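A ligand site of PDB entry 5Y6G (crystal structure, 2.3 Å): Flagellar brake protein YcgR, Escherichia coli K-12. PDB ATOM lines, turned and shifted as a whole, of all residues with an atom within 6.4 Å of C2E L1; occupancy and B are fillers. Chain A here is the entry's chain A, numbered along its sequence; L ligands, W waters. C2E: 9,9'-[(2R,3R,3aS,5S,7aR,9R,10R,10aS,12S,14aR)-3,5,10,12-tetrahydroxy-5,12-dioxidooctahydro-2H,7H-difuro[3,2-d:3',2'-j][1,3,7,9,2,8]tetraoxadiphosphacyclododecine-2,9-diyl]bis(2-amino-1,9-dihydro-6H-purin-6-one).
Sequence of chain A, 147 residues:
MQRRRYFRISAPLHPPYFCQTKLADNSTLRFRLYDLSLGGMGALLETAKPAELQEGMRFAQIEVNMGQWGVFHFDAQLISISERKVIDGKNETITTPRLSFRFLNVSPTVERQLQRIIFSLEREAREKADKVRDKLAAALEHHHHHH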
ATOM      1  N   GLN A   2       7.729   2.670  -5.139  1.00  0.00           N
ATOM      2  CA  GLN A   2       8.288   2.251  -3.853  1.00  0.00           C
ATOM      3  C   GLN A   2       7.335   2.595  -2.715  1.00  0.00           C
ATOM      4  O   GLN A   2       7.480   3.621  -2.057  1.00  0.00           O
ATOM      5  CB  GLN A   2       9.649   2.906  -3.626  1.00  0.00           C
ATOM      6  CG  GLN A   2       9.689   4.423  -3.852  1.00  0.00           C
ATOM      7  CD  GLN A   2       9.795   4.808  -5.312  1.00  0.00           C
ATOM      8  OE1 GLN A   2       9.946   3.959  -6.191  1.00  0.00           O
ATOM      9  NE2 GLN A   2       9.706   6.104  -5.592  1.00  0.00           N
ATOM     10  N   ARG A   3       6.355   1.724  -2.478  1.00  0.00           N
ATOM     11  CA  ARG A   3       5.339   2.022  -1.471  1.00  0.00           C
ATOM     12  C   ARG A   3       5.889   1.892  -0.054  1.00  0.00           C
ATOM     13  O   ARG A   3       5.476   2.637   0.840  1.00  0.00           O
ATOM     14  CB  ARG A   3       4.134   1.107  -1.657  1.00  0.00           C
ATOM     15  CG  ARG A   3       3.010   1.331  -0.659  1.00  0.00           C
ATOM     16  CD  ARG A   3       1.734   0.635  -1.091  1.00  0.00           C
ATOM     17  NE  ARG A   3       1.821  -0.824  -1.025  1.00  0.00           N
ATOM     18  CZ  ARG A   3       0.783  -1.636  -1.195  1.00  0.00           C
ATOM     19  NH1 ARG A   3      -0.411  -1.139  -1.444  1.00  0.00           N
ATOM     20  NH2 ARG A   3       0.953  -2.943  -1.120  1.00  0.00           N
ATOM     21  N   ARG A   4       6.814   0.965   0.171  1.00  0.00           N
ATOM     22  CA  ARG A   4       7.385   0.731   1.487  1.00  0.00           C
ATOM     23  C   ARG A   4       8.560   1.676   1.747  1.00  0.00           C
ATOM     24  O   ARG A   4       9.431   1.842   0.884  1.00  0.00           O
ATOM     25  CB  ARG A   4       7.846  -0.726   1.636  1.00  0.00           C
ATOM     26  CG  ARG A   4       6.710  -1.736   1.572  1.00  0.00           C
ATOM     27  CD  ARG A   4       7.237  -3.159   1.621  1.00  0.00           C
ATOM     28  NE  ARG A   4       6.167  -4.153   1.690  1.00  0.00           N
ATOM     29  CZ  ARG A   4       6.377  -5.458   1.706  1.00  0.00           C
ATOM     30  NH1 ARG A   4       7.619  -5.925   1.667  1.00  0.00           N
ATOM     31  NH2 ARG A   4       5.360  -6.305   1.757  1.00  0.00           N
ATOM     32  N   ARG A   8      12.508  -4.668   4.390  1.00  0.00           N
ATOM     33  CA  ARG A   8      12.085  -5.679   5.345  1.00  0.00           C
ATOM     34  C   ARG A   8      12.927  -6.932   5.182  1.00  0.00           C
ATOM     35  O   ARG A   8      13.007  -7.499   4.081  1.00  0.00           O
ATOM     36  CB  ARG A   8      10.598  -6.015   5.158  1.00  0.00           C
ATOM     37  CG  ARG A   8       9.689  -4.804   5.265  1.00  0.00           C
ATOM     38  CD  ARG A   8       8.233  -5.202   5.149  1.00  0.00           C
ATOM     39  NE  ARG A   8       7.361  -4.040   5.197  1.00  0.00           N
ATOM     40  CZ  ARG A   8       6.034  -4.101   5.213  1.00  0.00           C
ATOM     41  NH1 ARG A   8       5.421  -5.283   5.193  1.00  0.00           N
ATOM     42  NH2 ARG A   8       5.309  -2.991   5.254  1.00  0.00           N
ATOM     43  N   TYR A  34       8.093 -13.263  11.476  1.00  0.00           N
ATOM     44  CA  TYR A  34       8.111 -13.514  10.035  1.00  0.00           C
ATOM     45  C   TYR A  34       9.116 -12.627   9.309  1.00  0.00           C
ATOM     46  O   TYR A  34      10.023 -13.133   8.637  1.00  0.00           O
ATOM     47  CB  TYR A  34       6.711 -13.337   9.437  1.00  0.00           C
ATOM     48  CG  TYR A  34       6.631 -13.733   7.991  1.00  0.00           C
ATOM     49  CD1 TYR A  34       6.592 -15.063   7.606  1.00  0.00           C
ATOM     50  CD2 TYR A  34       6.608 -12.763   6.994  1.00  0.00           C
ATOM     51  CE1 TYR A  34       6.518 -15.432   6.274  1.00  0.00           C
ATOM     52  CE2 TYR A  34       6.537 -13.121   5.653  1.00  0.00           C
ATOM     53  CZ  TYR A  34       6.489 -14.450   5.309  1.00  0.00           C
ATOM     54  OH  TYR A  34       6.414 -14.809   3.977  1.00  0.00           O
ATOM     55  N   ASP A  35       8.982 -11.304   9.430  1.00  0.00           N
ATOM     56  CA  ASP A  35       9.977 -10.398   8.878  1.00  0.00           C
ATOM     57  C   ASP A  35      10.074  -9.191   9.803  1.00  0.00           C
ATOM     58  O   ASP A  35       9.251  -9.004  10.704  1.00  0.00           O
ATOM     59  CB  ASP A  35       9.644  -9.988   7.436  1.00  0.00           C
ATOM     60  CG  ASP A  35       8.323  -9.238   7.316  1.00  0.00           C
ATOM     61  OD1 ASP A  35       7.832  -8.679   8.315  1.00  0.00           O
ATOM     62  OD2 ASP A  35       7.759  -9.224   6.192  1.00  0.00           O
ATOM     63  N   ILE A  79      -1.781  -3.722  12.706  1.00  0.00           N
ATOM     64  CA  ILE A  79      -2.351  -3.002  11.574  1.00  0.00           C
ATOM     65  C   ILE A  79      -3.264  -3.887  10.718  1.00  0.00           C
ATOM     66  O   ILE A  79      -4.278  -3.412  10.200  1.00  0.00           O
ATOM     67  CB  ILE A  79      -1.230  -2.389  10.724  1.00  0.00           C
ATOM     68  CG1 ILE A  79      -0.482  -1.318  11.512  1.00  0.00           C
ATOM     69  CG2 ILE A  79      -1.799  -1.789   9.446  1.00  0.00           C
ATOM     70  CD1 ILE A  79      -1.373  -0.212  12.029  1.00  0.00           C
ATOM     71  N   SER A  80      -2.920  -5.165  10.544  1.00  0.00           N
ATOM     72  CA  SER A  80      -3.687  -5.994   9.626  1.00  0.00           C
ATOM     73  C   SER A  80      -3.524  -7.467   9.997  1.00  0.00           C
ATOM     74  O   SER A  80      -2.436  -7.900  10.372  1.00  0.00           O
ATOM     75  CB  SER A  80      -3.258  -5.769   8.178  1.00  0.00           C
ATOM     76  OG  SER A  80      -4.139  -6.420   7.273  1.00  0.00           O
ATOM     77  N   ILE A  81      -4.622  -8.223   9.886  1.00  0.00           N
ATOM     78  CA  ILE A  81      -4.609  -9.669  10.005  1.00  0.00           C
ATOM     79  C   ILE A  81      -4.928 -10.244   8.619  1.00  0.00           C
ATOM     80  O   ILE A  81      -6.020 -10.002   8.084  1.00  0.00           O
ATOM     81  CB  ILE A  81      -5.616 -10.175  11.045  1.00  0.00           C
ATOM     82  CG1 ILE A  81      -5.351  -9.537  12.405  1.00  0.00           C
ATOM     83  CG2 ILE A  81      -5.561 -11.697  11.150  1.00  0.00           C
ATOM     84  CD1 ILE A  81      -6.353  -9.930  13.470  1.00  0.00           C
ATOM     85  N   SER A  82      -3.981 -10.981   8.054  1.00  0.00           N
ATOM     86  CA  SER A  82      -4.193 -11.569   6.731  1.00  0.00           C
ATOM     87  C   SER A  82      -4.002 -13.076   6.781  1.00  0.00           C
ATOM     88  O   SER A  82      -3.840 -13.650   7.871  1.00  0.00           O
ATOM     89  CB  SER A  82      -3.248 -10.939   5.707  1.00  0.00           C
ATOM     90  OG  SER A  82      -1.891 -11.082   6.106  1.00  0.00           O
ATOM     91  N   GLU A  83      -4.028 -13.731   5.627  1.00  0.00           N
ATOM     92  CA  GLU A  83      -3.922 -15.177   5.536  1.00  0.00           C
ATOM     93  C   GLU A  83      -2.634 -15.565   4.829  1.00  0.00           C
ATOM     94  O   GLU A  83      -2.356 -15.087   3.721  1.00  0.00           O
ATOM     95  CB  GLU A  83      -5.116 -15.770   4.789  1.00  0.00           C
ATOM     96  CG  GLU A  83      -6.443 -15.598   5.508  1.00  0.00           C
ATOM     97  CD  GLU A  83      -7.580 -16.312   4.800  1.00  0.00           C
ATOM     98  OE1 GLU A  83      -7.592 -16.315   3.546  1.00  0.00           O
ATOM     99  OE2 GLU A  83      -8.436 -16.889   5.489  1.00  0.00           O
ATOM    100  N   ARG A  98      -1.746 -14.222   9.520  1.00  0.00           N
ATOM    101  CA  ARG A  98      -0.545 -13.407   9.380  1.00  0.00           C
ATOM    102  C   ARG A  98      -0.798 -12.041  10.001  1.00  0.00           C
ATOM    103  O   ARG A  98      -1.793 -11.380   9.684  1.00  0.00           O
ATOM    104  CB  ARG A  98      -0.155 -13.269   7.902  1.00  0.00           C
ATOM    105  CG  ARG A  98       0.723 -12.061   7.584  1.00  0.00           C
ATOM    106  CD  ARG A  98       2.095 -12.159   8.235  1.00  0.00           C
ATOM    107  NE  ARG A  98       2.892 -10.945   8.033  1.00  0.00           N
ATOM    108  CZ  ARG A  98       3.532 -10.653   6.913  1.00  0.00           C
ATOM    109  NH1 ARG A  98       3.487 -11.495   5.882  1.00  0.00           N
ATOM    110  NH2 ARG A  98       4.239  -9.536   6.811  1.00  0.00           N
ATOM    111  N   LEU A  99       0.105 -11.630  10.893  1.00  0.00           N
ATOM    112  CA  LEU A  99      -0.028 -10.374  11.605  1.00  0.00           C
ATOM    113  C   LEU A  99       0.924  -9.343  11.033  1.00  0.00           C
ATOM    114  O   LEU A  99       2.072  -9.667  10.704  1.00  0.00           O
ATOM    115  CB  LEU A  99       0.225 -10.569  13.099  1.00  0.00           C
ATOM    116  CG  LEU A  99      -0.573 -11.663  13.813  1.00  0.00           C
ATOM    117  CD1 LEU A  99      -0.237 -11.706  15.293  1.00  0.00           C
ATOM    118  CD2 LEU A  99      -2.082 -11.486  13.619  1.00  0.00           C
ATOM    119  N   SER A 100       0.443  -8.110  10.905  1.00  0.00           N
ATOM    120  CA  SER A 100       1.255  -7.001  10.432  1.00  0.00           C
ATOM    121  C   SER A 100       1.237  -5.913  11.489  1.00  0.00           C
ATOM    122  O   SER A 100       0.179  -5.319  11.753  1.00  0.00           O
ATOM    123  CB  SER A 100       0.740  -6.478   9.091  1.00  0.00           C
ATOM    124  OG  SER A 100       0.873  -7.478   8.090  1.00  0.00           O
HETATM  125  P1  C2E L   1       4.155 -10.179   2.297  1.00  0.00           P
HETATM  126  O2P C2E L   1       5.265  -9.026   2.438  1.00  0.00           O
HETATM  127  O1P C2E L   1       4.653 -11.433   2.901  1.00  0.00           O
HETATM  128  O5' C2E L   1       2.787  -9.731   3.009  1.00  0.00           O
HETATM  129  C5' C2E L   1       1.663 -10.589   3.098  1.00  0.00           C
HETATM  130  C4' C2E L   1       0.413  -9.818   3.536  1.00  0.00           C
HETATM  131  O4' C2E L   1       0.640  -9.142   4.778  1.00  0.00           O
HETATM  132  C3' C2E L   1       0.051  -8.700   2.541  1.00  0.00           C
HETATM  133  O3' C2E L   1      -0.682  -9.192   1.420  1.00  0.00           O
HETATM  134  C2' C2E L   1      -0.807  -7.790   3.441  1.00  0.00           C
HETATM  135  O2' C2E L   1      -2.149  -8.283   3.535  1.00  0.00           O
HETATM  136  C1' C2E L   1      -0.087  -7.913   4.785  1.00  0.00           C
HETATM  137  N9  C2E L   1       0.816  -6.768   4.914  1.00  0.00           N
HETATM  138  C8  C2E L   1       2.170  -6.782   4.754  1.00  0.00           C
HETATM  139  N7  C2E L   1       2.648  -5.587   4.953  1.00  0.00           N
HETATM  140  C5  C2E L   1       1.626  -4.744   5.248  1.00  0.00           C
HETATM  141  C6  C2E L   1       1.563  -3.361   5.550  1.00  0.00           C
HETATM  142  O6  C2E L   1       2.565  -2.674   5.579  1.00  0.00           O
HETATM  143  N1  C2E L   1       0.342  -2.829   5.800  1.00  0.00           N
HETATM  144  C2  C2E L   1      -0.770  -3.612   5.772  1.00  0.00           C
HETATM  145  N2  C2E L   1      -1.993  -3.029   6.033  1.00  0.00           N
HETATM  146  N3  C2E L   1      -0.724  -4.895   5.496  1.00  0.00           N
HETATM  147  C4  C2E L   1       0.446  -5.485   5.231  1.00  0.00           C
HETATM  148  P11 C2E L   1      -0.683  -8.425   0.010  1.00  0.00           P
HETATM  149  O21 C2E L   1      -0.960  -6.861   0.252  1.00  0.00           O
HETATM  150  O11 C2E L   1      -1.730  -9.004  -0.854  1.00  0.00           O
HETATM  151  O5A C2E L   1       0.762  -8.600  -0.696  1.00  0.00           O
HETATM  152  C5A C2E L   1       1.239  -9.874  -1.095  1.00  0.00           C
HETATM  153  C4A C2E L   1       2.750  -9.824  -1.366  1.00  0.00           C
HETATM  154  O4A C2E L   1       3.043  -8.864  -2.385  1.00  0.00           O
HETATM  155  C3A C2E L   1       3.535  -9.348  -0.141  1.00  0.00           C
HETATM  156  O3A C2E L   1       3.846 -10.429   0.740  1.00  0.00           O
HETATM  157  C2A C2E L   1       4.825  -8.813  -0.785  1.00  0.00           C
HETATM  158  O2A C2E L   1       5.733  -9.883  -1.071  1.00  0.00           O
HETATM  159  C1A C2E L   1       4.282  -8.200  -2.073  1.00  0.00           C
HETATM  160  N91 C2E L   1       4.041  -6.775  -1.858  1.00  0.00           N
HETATM  161  C81 C2E L   1       2.816  -6.186  -1.665  1.00  0.00           C
HETATM  162  N71 C2E L   1       2.973  -4.913  -1.501  1.00  0.00           N
HETATM  163  C51 C2E L   1       4.284  -4.595  -1.568  1.00  0.00           C
HETATM  164  C61 C2E L   1       5.009  -3.393  -1.459  1.00  0.00           C
HETATM  165  O61 C2E L   1       4.439  -2.325  -1.264  1.00  0.00           O
HETATM  166  N11 C2E L   1       6.357  -3.437  -1.577  1.00  0.00           N
HETATM  167  C21 C2E L   1       6.983  -4.630  -1.801  1.00  0.00           C
HETATM  168  N21 C2E L   1       8.350  -4.641  -1.921  1.00  0.00           N
HETATM  169  N31 C2E L   1       6.322  -5.763  -1.900  1.00  0.00           N
HETATM  170  C41 C2E L   1       4.987  -5.789  -1.788  1.00  0.00           C
HETATM  171  P1  C2E L   2       0.423   0.877   7.025  1.00  0.00           P
HETATM  172  O2P C2E L   2      -0.514  -0.400   6.778  1.00  0.00           O
HETATM  173  O1P C2E L   2      -0.311   1.878   7.829  1.00  0.00           O
HETATM  174  O5' C2E L   2       1.772   0.450   7.785  1.00  0.00           O
HETATM  175  C5' C2E L   2       2.690   1.408   8.310  1.00  0.00           C
HETATM  176  C4' C2E L   2       4.025   0.742   8.649  1.00  0.00           C
HETATM  177  O4' C2E L   2       3.832  -0.385   9.516  1.00  0.00           O
HETATM  178  C3' C2E L   2       4.717   0.175   7.403  1.00  0.00           C
HETATM  179  O3' C2E L   2       5.467   1.151   6.686  1.00  0.00           O
HETATM  180  C2' C2E L   2       5.653  -0.869   8.034  1.00  0.00           C
HETATM  181  O2' C2E L   2       6.886  -0.262   8.421  1.00  0.00           O
HETATM  182  C1' C2E L   2       4.861  -1.346   9.268  1.00  0.00           C
HETATM  183  N9  C2E L   2       4.293  -2.658   8.991  1.00  0.00           N
HETATM  184  C8  C2E L   2       2.970  -2.969   8.852  1.00  0.00           C
HETATM  185  N7  C2E L   2       2.844  -4.242   8.602  1.00  0.00           N
HETATM  186  C5  C2E L   2       4.069  -4.822   8.565  1.00  0.00           C
HETATM  187  C6  C2E L   2       4.531  -6.138   8.348  1.00  0.00           C
HETATM  188  O6  C2E L   2       3.760  -7.059   8.130  1.00  0.00           O
HETATM  189  N1  C2E L   2       5.864  -6.366   8.389  1.00  0.00           N
HETATM  190  C2  C2E L   2       6.726  -5.340   8.642  1.00  0.00           C
HETATM  191  N2  C2E L   2       8.067  -5.598   8.675  1.00  0.00           N
HETATM  192  N3  C2E L   2       6.307  -4.111   8.845  1.00  0.00           N
HETATM  193  C4  C2E L   2       5.001  -3.818   8.819  1.00  0.00           C
HETATM  194  P11 C2E L   2       5.890   0.937   5.143  1.00  0.00           P
HETATM  195  O21 C2E L   2       6.670  -0.465   4.993  1.00  0.00           O
HETATM  196  O11 C2E L   2       6.769   2.047   4.714  1.00  0.00           O
HETATM  197  O5A C2E L   2       4.555   0.933   4.242  1.00  0.00           O
HETATM  198  C5A C2E L   2       3.694   2.069   4.161  1.00  0.00           C
HETATM  199  C4A C2E L   2       2.303   1.696   3.631  1.00  0.00           C
HETATM  200  O4A C2E L   2       2.411   0.974   2.409  1.00  0.00           O
HETATM  201  C3A C2E L   2       1.562   0.777   4.609  1.00  0.00           C
HETATM  202  O3A C2E L   2       0.827   1.515   5.590  1.00  0.00           O
HETATM  203  C2A C2E L   2       0.591   0.050   3.659  1.00  0.00           C
HETATM  204  O2A C2E L   2      -0.605   0.815   3.510  1.00  0.00           O
HETATM  205  C1A C2E L   2       1.384  -0.012   2.343  1.00  0.00           C
HETATM  206  N91 C2E L   2       1.984  -1.347   2.194  1.00  0.00           N
HETATM  207  C81 C2E L   2       3.310  -1.654   2.275  1.00  0.00           C
HETATM  208  N71 C2E L   2       3.483  -2.934   2.106  1.00  0.00           N
HETATM  209  C51 C2E L   2       2.278  -3.527   1.911  1.00  0.00           C
HETATM  210  C61 C2E L   2       1.867  -4.865   1.689  1.00  0.00           C
HETATM  211  O61 C2E L   2       2.676  -5.784   1.623  1.00  0.00           O
HETATM  212  N11 C2E L   2       0.540  -5.108   1.536  1.00  0.00           N
HETATM  213  C21 C2E L   2      -0.355  -4.079   1.605  1.00  0.00           C
HETATM  214  N21 C2E L   2      -1.687  -4.362   1.450  1.00  0.00           N
HETATM  215  N31 C2E L   2       0.018  -2.836   1.819  1.00  0.00           N
HETATM  216  C41 C2E L   2       1.310  -2.528   1.977  1.00  0.00           C
HETATM  217  O   HOH W   1       6.020  -8.121   4.888  1.00  0.00           O
HETATM  218  O   HOH W   2       7.028 -12.331   2.802  1.00  0.00           O
HETATM  219  O   HOH W   3       3.489 -14.012   2.846  1.00  0.00           O
HETATM  220  O   HOH W   4      -3.256  -0.386   6.032  1.00  0.00           O
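Water W2 bridges an oxygen (O1P) of C2E L1 (2.5 Å) and the side-chain hydroxyl of Tyr 34 (2.8 Å).
Water W1 lies within hydrogen-bond range of OD2 of Asp 35 (2.4 Å), O2P of C2E L1 (2.7 Å), NH1 of Arg 8 (2.9 Å) and NH2 of Arg 98 (3.0 Å).
Water W3 bridges O1P of C2E L1 (2.8 Å) and OH of Tyr 34 (3.2 Å).
Water W4 bridges O2P of C2E L2 (2.8 Å) and N2 of C2E L1 (2.9 Å).
N9 of C2E L1 lies close to OG of Ser 100 (3.3 Å).
Residues that only touch C2E L1: Tyr 34, Ile 79 and Ser 80.
Hydrophobic or aromatic side chains within 4 Å of C2E L1: Tyr 34 and Ile 79.
Of the 14 residues printed, 9 come within 4 Å of C2E L1.
Along chain A the residues within 4 Å of C2E L1 span positions 3 to 100.
N of Ile 79 lies within hydrogen-bond range of O of Ser 100, at 2.7 Å.
The backbone NH (N) of Arg 98 lies within hydrogen-bond range of the backbone carbonyl oxygen (O) of Ser 82 (2.7 Å).
The backbone NH of Ser 100 is in hydrogen-bond range of the backbone carbonyl oxygen of Ser 80, 2.9 Å away.
The side-chain carboxylate of Asp 35 is in salt-bridge range of the guanidinium group of Arg 98 (3.6 Å).
A nitrogen (N11) of C2E L2 sits at hydrogen-bond distance from an oxygen (O21) of C2E L1, at 2.6 Å.
The guanidinium group (NH2) of Arg 3 lies within hydrogen-bond range of a nitrogen (N31) of C2E L2.
OD1 of Asp 35 is in hydrogen-bond range of N1 of C2E L2 (3.0 Å).
The guanidinium group (NH2) of Arg 98 sits at hydrogen-bond distance from an oxygen (O6) of C2E L2 (2.8 Å).
NH2 of Arg 8 lies within salt-bridge range of O21 of C2E L2, 2.9 Å away.
OG of Ser 82 is in hydrogen-bond range of O4' of C2E L1 (3.5 Å).
The guanidinium group of Arg 98 lies within salt-bridge range of an oxygen (O1P) of C2E L1.
NH2 of Arg 4 lies within salt-bridge range of O2P of C2E L1.
An oxygen (O6) of C2E L2 lies within hydrogen-bond range of the side-chain hydroxyl (OG) of Ser 100 (2.9 Å).
NH2 of Arg 8 lies within hydrogen-bond range of O6 of C2E L1.
The guanidinium group (NH2) of Arg 4 lies within hydrogen-bond range of an oxygen (O61) of C2E L2, at 2.7 Å.
The guanidinium group (NH2) of Arg 3 is in hydrogen-bond range of a nitrogen (N71) of C2E L1 (2.8 Å).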
